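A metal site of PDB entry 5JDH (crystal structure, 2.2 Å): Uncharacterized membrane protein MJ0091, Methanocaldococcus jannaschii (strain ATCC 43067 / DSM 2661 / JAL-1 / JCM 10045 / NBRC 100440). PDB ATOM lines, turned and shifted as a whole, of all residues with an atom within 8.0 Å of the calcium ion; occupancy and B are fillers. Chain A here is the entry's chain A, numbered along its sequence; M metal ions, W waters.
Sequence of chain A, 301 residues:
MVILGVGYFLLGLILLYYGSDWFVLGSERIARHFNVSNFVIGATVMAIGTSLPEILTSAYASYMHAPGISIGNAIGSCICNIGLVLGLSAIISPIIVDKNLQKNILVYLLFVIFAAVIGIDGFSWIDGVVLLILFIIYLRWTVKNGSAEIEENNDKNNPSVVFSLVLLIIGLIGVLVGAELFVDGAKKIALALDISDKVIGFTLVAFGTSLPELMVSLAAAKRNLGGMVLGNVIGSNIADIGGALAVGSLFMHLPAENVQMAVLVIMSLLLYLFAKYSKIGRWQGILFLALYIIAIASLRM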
ATOM      1  N   ALA A 115      -7.309 -26.882  20.546  1.00  0.00           N
ATOM      2  CA  ALA A 115      -8.633 -26.757  21.157  1.00  0.00           C
ATOM      3  C   ALA A 115      -8.725 -25.477  21.991  1.00  0.00           C
ATOM      4  O   ALA A 115      -9.738 -24.791  21.982  1.00  0.00           O
ATOM      5  CB  ALA A 115      -8.935 -27.970  22.023  1.00  0.00           C
ATOM      6  N   ALA A 116      -7.646 -25.163  22.695  1.00  0.00           N
ATOM      7  CA  ALA A 116      -7.617 -23.974  23.543  1.00  0.00           C
ATOM      8  C   ALA A 116      -7.727 -22.704  22.711  1.00  0.00           C
ATOM      9  O   ALA A 116      -8.470 -21.791  23.058  1.00  0.00           O
ATOM     10  CB  ALA A 116      -6.354 -23.952  24.387  1.00  0.00           C
ATOM     11  N   VAL A 117      -6.976 -22.657  21.618  1.00  0.00           N
ATOM     12  CA  VAL A 117      -6.934 -21.469  20.766  1.00  0.00           C
ATOM     13  C   VAL A 117      -8.300 -21.196  20.136  1.00  0.00           C
ATOM     14  O   VAL A 117      -8.783 -20.063  20.178  1.00  0.00           O
ATOM     15  CB  VAL A 117      -5.878 -21.598  19.656  1.00  0.00           C
ATOM     16  CG1 VAL A 117      -5.987 -20.434  18.689  1.00  0.00           C
ATOM     17  CG2 VAL A 117      -4.484 -21.655  20.262  1.00  0.00           C
ATOM     18  N   ILE A 118      -8.923 -22.218  19.562  1.00  0.00           N
ATOM     19  CA  ILE A 118     -10.217 -22.030  18.900  1.00  0.00           C
ATOM     20  C   ILE A 118     -11.332 -21.840  19.921  1.00  0.00           C
ATOM     21  O   ILE A 118     -12.442 -21.452  19.565  1.00  0.00           O
ATOM     22  CB  ILE A 118     -10.574 -23.213  17.979  1.00  0.00           C
ATOM     23  CG1 ILE A 118     -10.950 -24.451  18.792  1.00  0.00           C
ATOM     24  CG2 ILE A 118      -9.436 -23.505  17.001  1.00  0.00           C
ATOM     25  CD1 ILE A 118     -11.466 -25.615  17.954  1.00  0.00           C
ATOM     26  N   GLY A 119     -11.032 -22.098  21.186  1.00  0.00           N
ATOM     27  CA  GLY A 119     -12.027 -21.935  22.238  1.00  0.00           C
ATOM     28  C   GLY A 119     -11.936 -20.595  22.953  1.00  0.00           C
ATOM     29  O   GLY A 119     -12.711 -20.338  23.881  1.00  0.00           O
ATOM     30  N   ILE A 120     -11.014 -19.749  22.516  1.00  0.00           N
ATOM     31  CA  ILE A 120     -10.825 -18.424  23.112  1.00  0.00           C
ATOM     32  C   ILE A 120     -12.117 -17.603  23.049  1.00  0.00           C
ATOM     33  O   ILE A 120     -12.465 -16.900  23.996  1.00  0.00           O
ATOM     34  CB  ILE A 120      -9.679 -17.653  22.438  1.00  0.00           C
ATOM     35  CG1 ILE A 120      -8.340 -18.314  22.749  1.00  0.00           C
ATOM     36  CG2 ILE A 120      -9.657 -16.191  22.880  1.00  0.00           C
ATOM     37  CD1 ILE A 120      -7.167 -17.685  22.031  1.00  0.00           C
ATOM     38  N   ASP A 121     -12.825 -17.712  21.920  1.00  0.00           N
ATOM     39  CA  ASP A 121     -14.107 -17.052  21.755  1.00  0.00           C
ATOM     40  C   ASP A 121     -15.250 -18.034  21.957  1.00  0.00           C
ATOM     41  O   ASP A 121     -16.351 -17.837  21.449  1.00  0.00           O
ATOM     42  CB  ASP A 121     -14.200 -16.410  20.361  1.00  0.00           C
ATOM     43  CG  ASP A 121     -14.102 -17.437  19.242  1.00  0.00           C
ATOM     44  OD1 ASP A 121     -13.514 -18.516  19.470  1.00  0.00           O
ATOM     45  OD2 ASP A 121     -14.610 -17.162  18.135  1.00  0.00           O
ATOM     46  N   GLY A 122     -14.987 -19.104  22.705  1.00  0.00           N
ATOM     47  CA  GLY A 122     -15.977 -20.137  22.947  1.00  0.00           C
ATOM     48  C   GLY A 122     -15.937 -21.226  21.886  1.00  0.00           C
ATOM     49  O   GLY A 122     -15.114 -21.162  20.967  1.00  0.00           O
ATOM     50  N   PHE A 123     -16.808 -22.214  22.005  1.00  0.00           N
ATOM     51  CA  PHE A 123     -16.838 -23.335  21.072  1.00  0.00           C
ATOM     52  C   PHE A 123     -18.159 -23.404  20.316  1.00  0.00           C
ATOM     53  O   PHE A 123     -19.202 -23.680  20.894  1.00  0.00           O
ATOM     54  CB  PHE A 123     -16.602 -24.665  21.797  1.00  0.00           C
ATOM     55  CG  PHE A 123     -15.215 -24.825  22.348  1.00  0.00           C
ATOM     56  CD1 PHE A 123     -14.176 -25.286  21.539  1.00  0.00           C
ATOM     57  CD2 PHE A 123     -14.936 -24.512  23.674  1.00  0.00           C
ATOM     58  CE1 PHE A 123     -12.909 -25.434  22.050  1.00  0.00           C
ATOM     59  CE2 PHE A 123     -13.661 -24.666  24.185  1.00  0.00           C
ATOM     60  CZ  PHE A 123     -12.645 -25.123  23.368  1.00  0.00           C
ATOM     61  N   SER A 124     -18.090 -23.144  19.009  1.00  0.00           N
ATOM     62  CA  SER A 124     -19.255 -23.234  18.140  1.00  0.00           C
ATOM     63  C   SER A 124     -19.442 -24.662  17.660  1.00  0.00           C
ATOM     64  O   SER A 124     -18.557 -25.507  17.840  1.00  0.00           O
ATOM     65  CB  SER A 124     -19.108 -22.297  16.941  1.00  0.00           C
ATOM     66  OG  SER A 124     -18.026 -22.704  16.126  1.00  0.00           O
ATOM     67  N   TRP A 125     -20.589 -24.939  17.041  1.00  0.00           N
ATOM     68  CA  TRP A 125     -20.868 -26.272  16.543  1.00  0.00           C
ATOM     69  C   TRP A 125     -19.852 -26.683  15.472  1.00  0.00           C
ATOM     70  O   TRP A 125     -19.538 -27.863  15.317  1.00  0.00           O
ATOM     71  CB  TRP A 125     -22.290 -26.352  15.988  1.00  0.00           C
ATOM     72  CG  TRP A 125     -22.522 -25.461  14.814  1.00  0.00           C
ATOM     73  CD1 TRP A 125     -22.907 -24.153  14.828  1.00  0.00           C
ATOM     74  CD2 TRP A 125     -22.363 -25.828  13.433  1.00  0.00           C
ATOM     75  NE1 TRP A 125     -22.999 -23.678  13.543  1.00  0.00           N
ATOM     76  CE2 TRP A 125     -22.673 -24.673  12.674  1.00  0.00           C
ATOM     77  CE3 TRP A 125     -21.997 -26.995  12.770  1.00  0.00           C
ATOM     78  CZ2 TRP A 125     -22.631 -24.685  11.274  1.00  0.00           C
ATOM     79  CZ3 TRP A 125     -21.955 -26.992  11.389  1.00  0.00           C
ATOM     80  CH2 TRP A 125     -22.270 -25.843  10.651  1.00  0.00           C
ATOM     81  N   ILE A 126     -19.324 -25.692  14.750  1.00  0.00           N
ATOM     82  CA  ILE A 126     -18.253 -25.942  13.786  1.00  0.00           C
ATOM     83  C   ILE A 126     -16.969 -26.371  14.502  1.00  0.00           C
ATOM     84  O   ILE A 126     -16.253 -27.265  14.035  1.00  0.00           O
ATOM     85  CB  ILE A 126     -17.969 -24.702  12.921  1.00  0.00           C
ATOM     86  CG1 ILE A 126     -19.221 -24.293  12.143  1.00  0.00           C
ATOM     87  CG2 ILE A 126     -16.826 -24.957  11.961  1.00  0.00           C
ATOM     88  CD1 ILE A 126     -19.006 -23.152  11.169  1.00  0.00           C
ATOM     89  N   ASP A 127     -16.684 -25.731  15.629  1.00  0.00           N
ATOM     90  CA  ASP A 127     -15.531 -26.123  16.434  1.00  0.00           C
ATOM     91  C   ASP A 127     -15.665 -27.584  16.856  1.00  0.00           C
ATOM     92  O   ASP A 127     -14.691 -28.334  16.822  1.00  0.00           O
ATOM     93  CB  ASP A 127     -15.401 -25.234  17.672  1.00  0.00           C
ATOM     94  CG  ASP A 127     -15.013 -23.809  17.321  1.00  0.00           C
ATOM     95  OD1 ASP A 127     -14.308 -23.615  16.314  1.00  0.00           O
ATOM     96  OD2 ASP A 127     -15.404 -22.892  18.069  1.00  0.00           O
ATOM     97  N   GLY A 128     -16.869 -27.974  17.253  1.00  0.00           N
ATOM     98  CA  GLY A 128     -17.137 -29.345  17.661  1.00  0.00           C
ATOM     99  C   GLY A 128     -16.900 -30.341  16.538  1.00  0.00           C
ATOM    100  O   GLY A 128     -16.281 -31.381  16.761  1.00  0.00           O
ATOM    101  N   HIS A 253     -23.710 -23.141  21.497  1.00  0.00           N
ATOM    102  CA  HIS A 253     -22.404 -22.521  21.652  1.00  0.00           C
ATOM    103  C   HIS A 253     -21.941 -22.630  23.105  1.00  0.00           C
ATOM    104  O   HIS A 253     -22.684 -22.284  24.026  1.00  0.00           O
ATOM    105  CB  HIS A 253     -22.449 -21.062  21.226  1.00  0.00           C
ATOM    106  CG  HIS A 253     -21.130 -20.358  21.325  1.00  0.00           C
ATOM    107  ND1 HIS A 253     -20.220 -20.338  20.290  1.00  0.00           N
ATOM    108  CD2 HIS A 253     -20.562 -19.659  22.334  1.00  0.00           C
ATOM    109  CE1 HIS A 253     -19.151 -19.661  20.664  1.00  0.00           C
ATOM    110  NE2 HIS A 253     -19.338 -19.240  21.894  1.00  0.00           N
ATOM    111  N   LEU A 254     -20.725 -23.118  23.308  1.00  0.00           N
ATOM    112  CA  LEU A 254     -20.182 -23.264  24.646  1.00  0.00           C
ATOM    113  C   LEU A 254     -19.367 -22.034  25.011  1.00  0.00           C
ATOM    114  O   LEU A 254     -18.494 -21.622  24.250  1.00  0.00           O
ATOM    115  CB  LEU A 254     -19.326 -24.529  24.750  1.00  0.00           C
ATOM    116  CG  LEU A 254     -19.948 -25.828  24.220  1.00  0.00           C
ATOM    117  CD1 LEU A 254     -19.001 -26.999  24.422  1.00  0.00           C
ATOM    118  CD2 LEU A 254     -21.291 -26.103  24.884  1.00  0.00           C
ATOM    119  N   ALA A 256     -16.569 -19.606  26.568  1.00  0.00           N
ATOM    120  CA  ALA A 256     -15.130 -19.791  26.715  1.00  0.00           C
ATOM    121  C   ALA A 256     -14.728 -19.978  28.178  1.00  0.00           C
ATOM    122  O   ALA A 256     -15.218 -19.274  29.057  1.00  0.00           O
ATOM    123  CB  ALA A 256     -14.392 -18.605  26.125  1.00  0.00           C
HETATM  124 CA    CA M   1     -14.439 -20.676  18.711  1.00  0.00          CA
HETATM  125  O   HOH W   1     -13.132 -20.816  16.283  1.00  0.00           O
HETATM  126  O   HOH W   2     -16.644 -20.006  17.952  1.00  0.00           O
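A ring nitrogen (NE2) of His 253 is in hydrogen-bond range of the backbone carbonyl oxygen (O) of Asp 121, 3.3 Å away.
The backbone NH (N) of Asp 127 is in hydrogen-bond range of the side-chain hydroxyl (OG) of Ser 124 (3.3 Å).
Four residues have an atom within 4 Å of the calcium ion: Ile 118, Asp 121, Gly 122 and Asp 127.
The nearest printed residue that does not touch the calcium ion is Phe 123 (4.3 Å).
The calcium ion is bound by O of Ile 118, O of Gly 122, water W2, OD1 of Asp 121, OD2 of Asp 127 and water W1.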
